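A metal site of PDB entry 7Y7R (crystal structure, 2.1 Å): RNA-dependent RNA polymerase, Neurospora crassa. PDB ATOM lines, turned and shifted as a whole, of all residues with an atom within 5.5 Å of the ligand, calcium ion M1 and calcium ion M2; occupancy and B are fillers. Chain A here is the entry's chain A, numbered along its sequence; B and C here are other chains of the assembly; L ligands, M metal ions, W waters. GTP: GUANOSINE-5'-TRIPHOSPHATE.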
ATOM      1  N   ARG A 295      24.756  20.887   0.623  1.00  0.00           N
ATOM      2  CA  ARG A 295      25.163  21.149   2.001  1.00  0.00           C
ATOM      3  C   ARG A 295      26.614  21.627   2.110  1.00  0.00           C
ATOM      4  O   ARG A 295      27.022  22.031   3.206  1.00  0.00           O
ATOM      5  CB  ARG A 295      24.974  19.909   2.864  1.00  0.00           C
ATOM      6  CG  ARG A 295      23.550  19.374   2.874  1.00  0.00           C
ATOM      7  CD  ARG A 295      22.546  20.494   3.021  1.00  0.00           C
ATOM      8  NE  ARG A 295      21.199  19.980   3.258  1.00  0.00           N
ATOM      9  CZ  ARG A 295      20.143  20.749   3.498  1.00  0.00           C
ATOM     10  NH1 ARG A 295      20.259  22.066   3.579  1.00  0.00           N
ATOM     11  NH2 ARG A 295      18.951  20.185   3.643  1.00  0.00           N
ATOM     12  N   ASP A 333      10.823  23.243  13.559  1.00  0.00           N
ATOM     13  CA  ASP A 333      11.707  23.016  12.433  1.00  0.00           C
ATOM     14  C   ASP A 333      12.862  24.003  12.402  1.00  0.00           C
ATOM     15  O   ASP A 333      12.645  25.194  12.132  1.00  0.00           O
ATOM     16  CB  ASP A 333      10.869  23.095  11.148  1.00  0.00           C
ATOM     17  CG  ASP A 333      11.625  22.663   9.897  1.00  0.00           C
ATOM     18  OD1 ASP A 333      12.872  22.517   9.909  1.00  0.00           O
ATOM     19  OD2 ASP A 333      10.929  22.504   8.867  1.00  0.00           O
ATOM     20  N   LYS A 367      22.078  23.314  11.333  1.00  0.00           N
ATOM     21  CA  LYS A 367      21.930  24.676  10.851  1.00  0.00           C
ATOM     22  C   LYS A 367      20.647  25.220  11.447  1.00  0.00           C
ATOM     23  O   LYS A 367      19.650  24.503  11.528  1.00  0.00           O
ATOM     24  CB  LYS A 367      21.885  24.709   9.285  1.00  0.00           C
ATOM     25  CG  LYS A 367      21.802  26.095   8.650  1.00  0.00           C
ATOM     26  CD  LYS A 367      21.330  26.056   7.198  1.00  0.00           C
ATOM     27  CE  LYS A 367      20.127  25.141   7.039  1.00  0.00           C
ATOM     28  NZ  LYS A 367      18.784  25.833   7.148  1.00  0.00           N
ATOM     29  N   SER A 388      15.421  18.180  12.641  1.00  0.00           N
ATOM     30  CA  SER A 388      15.148  19.192  11.624  1.00  0.00           C
ATOM     31  C   SER A 388      16.359  20.088  11.401  1.00  0.00           C
ATOM     32  O   SER A 388      16.514  20.657  10.322  1.00  0.00           O
ATOM     33  CB  SER A 388      13.944  20.042  12.001  1.00  0.00           C
ATOM     34  OG  SER A 388      14.168  20.727  13.229  1.00  0.00           O
ATOM     35  N   LYS A 391      21.688  18.419   9.010  1.00  0.00           N
ATOM     36  CA  LYS A 391      21.506  18.236   7.580  1.00  0.00           C
ATOM     37  C   LYS A 391      22.276  17.049   7.039  1.00  0.00           C
ATOM     38  O   LYS A 391      22.120  16.698   5.866  1.00  0.00           O
ATOM     39  CB  LYS A 391      21.910  19.515   6.835  1.00  0.00           C
ATOM     40  CG  LYS A 391      21.084  20.742   7.162  1.00  0.00           C
ATOM     41  CD  LYS A 391      19.596  20.446   7.223  1.00  0.00           C
ATOM     42  CE  LYS A 391      18.788  21.733   7.406  1.00  0.00           C
ATOM     43  NZ  LYS A 391      17.362  21.438   7.744  1.00  0.00           N
ATOM     44  N   ARG A 586       6.122  36.362   5.383  1.00  0.00           N
ATOM     45  CA  ARG A 586       7.482  36.223   4.911  1.00  0.00           C
ATOM     46  C   ARG A 586       7.550  36.695   3.463  1.00  0.00           C
ATOM     47  O   ARG A 586       6.578  36.603   2.708  1.00  0.00           O
ATOM     48  CB  ARG A 586       7.950  34.770   5.067  1.00  0.00           C
ATOM     49  CG  ARG A 586       9.423  34.650   5.407  1.00  0.00           C
ATOM     50  CD  ARG A 586       9.751  33.328   6.060  1.00  0.00           C
ATOM     51  NE  ARG A 586       9.409  32.215   5.181  1.00  0.00           N
ATOM     52  CZ  ARG A 586      10.182  31.741   4.210  1.00  0.00           C
ATOM     53  NH1 ARG A 586      11.399  32.199   3.991  1.00  0.00           N
ATOM     54  NH2 ARG A 586       9.699  30.775   3.433  1.00  0.00           N
ATOM     55  N   SER A 587       8.695  37.239   3.091  1.00  0.00           N
ATOM     56  CA  SER A 587       9.036  37.398   1.680  1.00  0.00           C
ATOM     57  C   SER A 587       9.782  36.155   1.189  1.00  0.00           C
ATOM     58  O   SER A 587      10.671  35.662   1.896  1.00  0.00           O
ATOM     59  CB  SER A 587       9.906  38.617   1.481  1.00  0.00           C
ATOM     60  OG  SER A 587       9.120  39.785   1.680  1.00  0.00           O
ATOM     61  N   PRO A 588       9.440  35.600   0.015  1.00  0.00           N
ATOM     62  CA  PRO A 588       8.444  36.089  -0.946  1.00  0.00           C
ATOM     63  C   PRO A 588       7.024  35.710  -0.552  1.00  0.00           C
ATOM     64  O   PRO A 588       6.808  34.564  -0.155  1.00  0.00           O
ATOM     65  CB  PRO A 588       8.841  35.377  -2.246  1.00  0.00           C
ATOM     66  CG  PRO A 588       9.390  34.051  -1.789  1.00  0.00           C
ATOM     67  CD  PRO A 588      10.017  34.301  -0.413  1.00  0.00           C
ATOM     68  N   SER A 628       4.651  31.128   3.491  1.00  0.00           N
ATOM     69  CA  SER A 628       5.452  30.770   2.330  1.00  0.00           C
ATOM     70  C   SER A 628       6.356  29.577   2.620  1.00  0.00           C
ATOM     71  O   SER A 628       7.503  29.525   2.167  1.00  0.00           O
ATOM     72  CB  SER A 628       6.260  31.988   1.853  1.00  0.00           C
ATOM     73  OG  SER A 628       6.774  31.788   0.550  1.00  0.00           O
ATOM     74  N   GLY A 630       7.738  28.622   5.504  1.00  0.00           N
ATOM     75  CA  GLY A 630       8.872  28.997   6.338  1.00  0.00           C
ATOM     76  C   GLY A 630       9.062  28.105   7.550  1.00  0.00           C
ATOM     77  O   GLY A 630       8.381  27.094   7.736  1.00  0.00           O
ATOM     78  N   ASP A 631      10.032  28.476   8.381  1.00  0.00           N
ATOM     79  CA  ASP A 631      10.348  27.680   9.557  1.00  0.00           C
ATOM     80  C   ASP A 631      11.207  28.529  10.494  1.00  0.00           C
ATOM     81  O   ASP A 631      11.226  29.761  10.388  1.00  0.00           O
ATOM     82  CB  ASP A 631      11.019  26.357   9.147  1.00  0.00           C
ATOM     83  CG  ASP A 631      12.221  26.571   8.255  1.00  0.00           C
ATOM     84  OD1 ASP A 631      12.832  27.656   8.289  1.00  0.00           O
ATOM     85  OD2 ASP A 631      12.557  25.616   7.519  1.00  0.00           O
ATOM     86  N   ASP A 633      14.674  28.426  11.137  1.00  0.00           N
ATOM     87  CA  ASP A 633      16.123  28.228  10.967  1.00  0.00           C
ATOM     88  C   ASP A 633      16.837  29.481  10.492  1.00  0.00           C
ATOM     89  O   ASP A 633      17.944  29.386   9.963  1.00  0.00           O
ATOM     90  CB  ASP A 633      16.392  27.067  10.014  1.00  0.00           C
ATOM     91  CG  ASP A 633      15.992  27.371   8.582  1.00  0.00           C
ATOM     92  OD1 ASP A 633      15.476  28.486   8.313  1.00  0.00           O
ATOM     93  OD2 ASP A 633      16.182  26.484   7.720  1.00  0.00           O
ATOM     94  N   GLY A 634      16.248  30.657  10.681  1.00  0.00           N
ATOM     95  CA  GLY A 634      16.892  31.869  10.225  1.00  0.00           C
ATOM     96  C   GLY A 634      15.913  32.739   9.464  1.00  0.00           C
ATOM     97  O   GLY A 634      16.184  33.909   9.195  1.00  0.00           O
ATOM     98  N   ASP A 635      14.768  32.150   9.110  1.00  0.00           N
ATOM     99  CA  ASP A 635      13.665  32.908   8.537  1.00  0.00           C
ATOM    100  C   ASP A 635      13.344  34.125   9.411  1.00  0.00           C
ATOM    101  O   ASP A 635      13.360  34.033  10.646  1.00  0.00           O
ATOM    102  CB  ASP A 635      12.406  32.017   8.434  1.00  0.00           C
ATOM    103  CG  ASP A 635      12.503  30.947   7.315  1.00  0.00           C
ATOM    104  OD1 ASP A 635      13.583  30.726   6.690  1.00  0.00           O
ATOM    105  OD2 ASP A 635      11.468  30.298   7.065  1.00  0.00           O
ATOM    106  N   LEU A 706      13.452  30.482 -12.047  1.00  0.00           N
ATOM    107  CA  LEU A 706      12.836  31.230 -10.963  1.00  0.00           C
ATOM    108  C   LEU A 706      12.484  32.646 -11.413  1.00  0.00           C
ATOM    109  O   LEU A 706      11.369  33.114 -11.206  1.00  0.00           O
ATOM    110  CB  LEU A 706      13.771  31.266  -9.761  1.00  0.00           C
ATOM    111  CG  LEU A 706      13.221  32.025  -8.582  1.00  0.00           C
ATOM    112  CD1 LEU A 706      11.832  31.513  -8.214  1.00  0.00           C
ATOM    113  CD2 LEU A 706      14.189  31.906  -7.446  1.00  0.00           C
ATOM    114  N   VAL A 739      12.271  27.806  -6.016  1.00  0.00           N
ATOM    115  CA  VAL A 739      13.288  28.337  -5.101  1.00  0.00           C
ATOM    116  C   VAL A 739      14.076  27.205  -4.467  1.00  0.00           C
ATOM    117  O   VAL A 739      15.263  27.358  -4.184  1.00  0.00           O
ATOM    118  CB  VAL A 739      12.718  29.267  -4.012  1.00  0.00           C
ATOM    119  CG1 VAL A 739      12.519  30.681  -4.520  1.00  0.00           C
ATOM    120  CG2 VAL A 739      11.431  28.716  -3.424  1.00  0.00           C
ATOM    121  N   ASP A 740      13.429  26.068  -4.226  1.00  0.00           N
ATOM    122  CA  ASP A 740      14.033  24.887  -3.610  1.00  0.00           C
ATOM    123  C   ASP A 740      14.844  24.050  -4.601  1.00  0.00           C
ATOM    124  O   ASP A 740      15.218  22.919  -4.284  1.00  0.00           O
ATOM    125  CB  ASP A 740      12.932  23.999  -2.997  1.00  0.00           C
ATOM    126  CG  ASP A 740      12.016  24.766  -2.025  1.00  0.00           C
ATOM    127  OD1 ASP A 740      12.259  25.963  -1.779  1.00  0.00           O
ATOM    128  OD2 ASP A 740      11.026  24.163  -1.552  1.00  0.00           O
ATOM    129  N   LYS A 743      18.625  22.409  -4.101  1.00  0.00           N
ATOM    130  CA  LYS A 743      18.556  21.554  -2.943  1.00  0.00           C
ATOM    131  C   LYS A 743      17.580  20.387  -3.125  1.00  0.00           C
ATOM    132  O   LYS A 743      17.735  19.357  -2.472  1.00  0.00           O
ATOM    133  CB  LYS A 743      18.166  22.376  -1.708  1.00  0.00           C
ATOM    134  CG  LYS A 743      18.847  21.983  -0.433  1.00  0.00           C
ATOM    135  CD  LYS A 743      18.461  22.900   0.730  1.00  0.00           C
ATOM    136  CE  LYS A 743      19.157  24.245   0.647  1.00  0.00           C
ATOM    137  NZ  LYS A 743      18.639  25.143   1.716  1.00  0.00           N
ATOM    138  P    DC B   7      15.624  38.281 -12.635  1.00  0.00           P
ATOM    139  OP1  DC B   7      15.510  39.655 -13.173  1.00  0.00           O
ATOM    140  OP2  DC B   7      16.894  37.816 -12.040  1.00  0.00           O
ATOM    141  O5'  DC B   7      14.490  38.054 -11.538  1.00  0.00           O
ATOM    142  C5'  DC B   7      13.177  38.546 -11.742  1.00  0.00           C
ATOM    143  C4'  DC B   7      12.368  38.386 -10.461  1.00  0.00           C
ATOM    144  O4'  DC B   7      12.430  37.004 -10.044  1.00  0.00           O
ATOM    145  C3'  DC B   7      12.895  39.169  -9.271  1.00  0.00           C
ATOM    146  O3'  DC B   7      12.348  40.489  -9.281  1.00  0.00           O
ATOM    147  C2'  DC B   7      12.377  38.356  -8.087  1.00  0.00           C
ATOM    148  C1'  DC B   7      12.488  36.931  -8.623  1.00  0.00           C
ATOM    149  N1   DC B   7      13.774  36.256  -8.239  1.00  0.00           N
ATOM    150  C2   DC B   7      13.912  35.760  -6.936  1.00  0.00           C
ATOM    151  O2   DC B   7      12.973  35.901  -6.127  1.00  0.00           O
ATOM    152  N3   DC B   7      15.072  35.135  -6.585  1.00  0.00           N
ATOM    153  C4   DC B   7      16.052  35.014  -7.484  1.00  0.00           C
ATOM    154  N4   DC B   7      17.183  34.411  -7.086  1.00  0.00           N
ATOM    155  C5   DC B   7      15.932  35.517  -8.826  1.00  0.00           C
ATOM    156  C6   DC B   7      14.781  36.120  -9.144  1.00  0.00           C
ATOM    157  P    DC B   8      13.067  41.658  -8.434  1.00  0.00           P
ATOM    158  OP1  DC B   8      12.473  42.950  -8.839  1.00  0.00           O
ATOM    159  OP2  DC B   8      14.526  41.447  -8.519  1.00  0.00           O
ATOM    160  O5'  DC B   8      12.646  41.343  -6.926  1.00  0.00           O
ATOM    161  C5'  DC B   8      11.281  41.417  -6.537  1.00  0.00           C
ATOM    162  C4'  DC B   8      11.082  40.802  -5.159  1.00  0.00           C
ATOM    163  O4'  DC B   8      11.481  39.412  -5.164  1.00  0.00           O
ATOM    164  C3'  DC B   8      11.891  41.432  -4.039  1.00  0.00           C
ATOM    165  O3'  DC B   8      11.216  42.539  -3.587  1.00  0.00           O
ATOM    166  C2'  DC B   8      11.886  40.333  -3.004  1.00  0.00           C
ATOM    167  C1'  DC B   8      11.943  39.071  -3.862  1.00  0.00           C
ATOM    168  N1   DC B   8      13.313  38.443  -3.938  1.00  0.00           N
ATOM    169  C2   DC B   8      13.688  37.568  -2.925  1.00  0.00           C
ATOM    170  O2   DC B   8      12.878  37.336  -2.003  1.00  0.00           O
ATOM    171  N3   DC B   8      14.910  36.977  -2.983  1.00  0.00           N
ATOM    172  C4   DC B   8      15.733  37.245  -3.990  1.00  0.00           C
ATOM    173  N4   DC B   8      16.920  36.628  -3.990  1.00  0.00           N
ATOM    174  C5   DC B   8      15.366  38.133  -5.051  1.00  0.00           C
ATOM    175  C6   DC B   8      14.157  38.720  -4.975  1.00  0.00           C
ATOM    176  P     G C   7      20.627  30.695   5.048  1.00  0.00           P
ATOM    177  OP1   G C   7      20.500  29.584   6.027  1.00  0.00           O
ATOM    178  OP2   G C   7      21.256  30.441   3.719  1.00  0.00           O
ATOM    179  O5'   G C   7      19.209  31.410   4.931  1.00  0.00           O
ATOM    180  C5'   G C   7      18.403  31.638   6.096  1.00  0.00           C
ATOM    181  C4'   G C   7      17.046  32.177   5.717  1.00  0.00           C
ATOM    182  O4'   G C   7      17.190  33.451   5.043  1.00  0.00           O
ATOM    183  C3'   G C   7      16.224  31.324   4.758  1.00  0.00           C
ATOM    184  C2'   G C   7      15.275  32.346   4.120  1.00  0.00           C
ATOM    185  O2'   G C   7      14.154  32.614   4.972  1.00  0.00           O
ATOM    186  C1'   G C   7      16.175  33.591   4.067  1.00  0.00           C
ATOM    187  N9    G C   7      16.821  33.808   2.752  1.00  0.00           N
ATOM    188  C8    G C   7      18.066  33.428   2.350  1.00  0.00           C
ATOM    189  N7    G C   7      18.354  33.807   1.127  1.00  0.00           N
ATOM    190  C5    G C   7      17.209  34.480   0.720  1.00  0.00           C
ATOM    191  C6    G C   7      16.919  35.114  -0.519  1.00  0.00           C
ATOM    192  O6    G C   7      17.641  35.189  -1.513  1.00  0.00           O
ATOM    193  N1    G C   7      15.645  35.689  -0.506  1.00  0.00           N
ATOM    194  C2    G C   7      14.782  35.654   0.556  1.00  0.00           C
ATOM    195  N2    G C   7      13.609  36.261   0.383  1.00  0.00           N
ATOM    196  N3    G C   7      15.035  35.062   1.714  1.00  0.00           N
ATOM    197  C4    G C   7      16.261  34.496   1.714  1.00  0.00           C
HETATM  198  PG  GTP L   1      16.806  23.306   4.530  1.00  0.00           P
HETATM  199  O1G GTP L   1      18.101  23.995   4.149  1.00  0.00           O
HETATM  200  O2G GTP L   1      17.001  21.817   4.426  1.00  0.00           O
HETATM  201  O3G GTP L   1      16.418  23.684   5.931  1.00  0.00           O
HETATM  202  O3B GTP L   1      15.582  23.735   3.534  1.00  0.00           O
HETATM  203  PB  GTP L   1      14.831  25.178   3.543  1.00  0.00           P
HETATM  204  O1B GTP L   1      13.754  25.240   2.494  1.00  0.00           O
HETATM  205  O2B GTP L   1      14.295  25.587   4.889  1.00  0.00           O
HETATM  206  O3A GTP L   1      16.042  26.162   3.133  1.00  0.00           O
HETATM  207  PA  GTP L   1      16.098  27.696   3.619  1.00  0.00           P
HETATM  208  O1A GTP L   1      17.368  28.307   3.090  1.00  0.00           O
HETATM  209  O2A GTP L   1      16.005  27.844   5.120  1.00  0.00           O
HETATM  210  O5' GTP L   1      14.790  28.402   3.012  1.00  0.00           O
HETATM  211  C5' GTP L   1      14.258  28.205   1.725  1.00  0.00           C
HETATM  212  C4' GTP L   1      13.480  29.491   1.421  1.00  0.00           C
HETATM  213  O4' GTP L   1      14.321  30.635   1.405  1.00  0.00           O
HETATM  214  C3' GTP L   1      12.749  29.512   0.081  1.00  0.00           C
HETATM  215  C2' GTP L   1      12.588  31.009  -0.093  1.00  0.00           C
HETATM  216  O2' GTP L   1      11.447  31.397   0.626  1.00  0.00           O
HETATM  217  C1' GTP L   1      13.790  31.647   0.564  1.00  0.00           C
HETATM  218  N9  GTP L   1      14.765  31.899  -0.499  1.00  0.00           N
HETATM  219  C8  GTP L   1      16.054  31.423  -0.524  1.00  0.00           C
HETATM  220  N7  GTP L   1      16.639  31.840  -1.677  1.00  0.00           N
HETATM  221  C5  GTP L   1      15.744  32.576  -2.385  1.00  0.00           C
HETATM  222  C6  GTP L   1      15.806  33.239  -3.612  1.00  0.00           C
HETATM  223  O6  GTP L   1      16.835  33.224  -4.291  1.00  0.00           O
HETATM  224  N1  GTP L   1      14.710  33.910  -4.076  1.00  0.00           N
HETATM  225  C2  GTP L   1      13.549  33.947  -3.350  1.00  0.00           C
HETATM  226  N2  GTP L   1      12.490  34.596  -3.810  1.00  0.00           N
HETATM  227  N3  GTP L   1      13.491  33.289  -2.136  1.00  0.00           N
HETATM  228  C4  GTP L   1      14.553  32.613  -1.660  1.00  0.00           C
HETATM  229 CA    CA M   1      14.124  28.199   6.309  1.00  0.00          CA
HETATM  230 CA    CA M   2      14.726  24.785   6.860  1.00  0.00          CA
HETATM  231 MG    MG M   3      11.188  25.596   4.811  1.00  0.00          MG
HETATM  232  O   HOH W   1      12.982  23.195   6.420  1.00  0.00           O
HETATM  233  O   HOH W   2      19.168  30.194   1.670  1.00  0.00           O
HETATM  234  O   HOH W   3       9.159  30.226  -0.392  1.00  0.00           O
HETATM  235  O   HOH W   4      14.950  23.759   8.958  1.00  0.00           O
HETATM  236  O   HOH W   5      19.159  30.643  -2.005  1.00  0.00           O
HETATM  237  O   HOH W   6      12.208  28.190   5.088  1.00  0.00           O
HETATM  238  O   HOH W   7      19.408  33.883  -2.820  1.00  0.00           O
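The guanidinium group of Arg 295 lies within salt-bridge range of an oxygen (O2G) of the ligand (2.7 Å).
O2 of DC 7 of chain B lies within hydrogen-bond range of a nitrogen (N2) of the ligand (2.7 Å).
The side-chain amino group of Lys 743 lies within salt-bridge range of an oxygen (O1G) of the ligand, 2.7 Å away.
The side-chain amino group of Lys 391 lies within salt-bridge range of an oxygen (O2G) of the ligand (3.4 Å).
N3 of DC 8 of chain B sits at hydrogen-bond distance from N1 of the ligand, at 3.3 Å.
O2' of the ligand lies within hydrogen-bond range of NH2 of Arg 586 (3.4 Å).
O1G of the ligand lies within salt-bridge range of NZ of Lys 367.
The side-chain carboxylate (OD2) of Asp 633 sits close to the side-chain amino group (NZ) of Lys 367 (2.7 Å).
O2' of G 7 of chain C lies close to OD1 of Asp 635.
The side-chain carboxylate (OD2) of Asp 635 lies within salt-bridge range of the guanidinium group (NE) of Arg 586 (3.4 Å).
O of Ser 388 sits at hydrogen-bond distance from NZ of Lys 391 (2.8 Å).
O2 of DC 8 of chain B sits close to N2 of G 7 of chain C (2.7 Å).
The guanidinium group of Arg 586 sits at hydrogen-bond distance from O2' of G 7 of chain C.
The guanidinium group (NH2) of Arg 586 sits at hydrogen-bond distance from the backbone carbonyl oxygen (O) of Ser 628, 2.8 Å away.
The backbone carbonyl oxygen (O) of Pro 588 is in hydrogen-bond range of the side-chain hydroxyl (OG) of Ser 628 (2.9 Å).
O6 of G 7 of chain C lies close to an oxygen (O6) of the ligand.
Pro 588 touches the ligand (CD to O2', 3.4 Å).
CD2 of Leu 706 touches N1 of the ligand, 3.96 Å away.
CG1 of Val 739 touches C2 of the ligand (3.6 Å).
Hydrophobic or aromatic side chains that line the ligand: Pro 588, Leu 706 and Val 739.
Of the 21 residues printed, 13 come within 4 Å of the ligand.
Of the 21 residues printed, 2 come within 4 Å of calcium ion M2.
Calcium ion M1 is bound by O2A of the ligand (2.3 Å), water W6 (2.3 Å), OD1 of Asp 631 (2.4 Å), OD1 of Asp 633 (2.4 Å) and OD1 of Asp 635 (2.6 Å).
Calcium ion M1 has five donor atoms within binding distance.
Slightly farther from calcium ion M1 lies an oxygen (O2B) of the ligand (3.0 Å).
Slightly farther from calcium ion M1 lies OD2 of Asp 633 (3.0 Å).
Calcium ion M2 is bound by O2B of the ligand.
O3G of the ligand is bound to calcium ion M2 (2.2 Å).
Water W4 binds calcium ion M2 (2.3 Å).
OD2 of Asp 633 binds calcium ion M2 (2.4 Å).
Water W1 is bound to calcium ion M2, at 2.4 Å.
Calcium ion M2 is bound by OD2 of Asp 631 (2.4 Å).
Water W6 bridges OD2 of Asp 635 (3.0 Å) and O5' of the ligand (3.3 Å).
Water W3 lies within hydrogen-bond range of O2' of the ligand (2.8 Å) and OG of Ser 628 (3.0 Å).
Water W2 bridges OP2 of G 7 of chain C (2.9 Å) and an oxygen (O1A) of the ligand (3.0 Å).
Water W7 lies within hydrogen-bond range of O6 of G 7 of chain C and O6 of the ligand.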
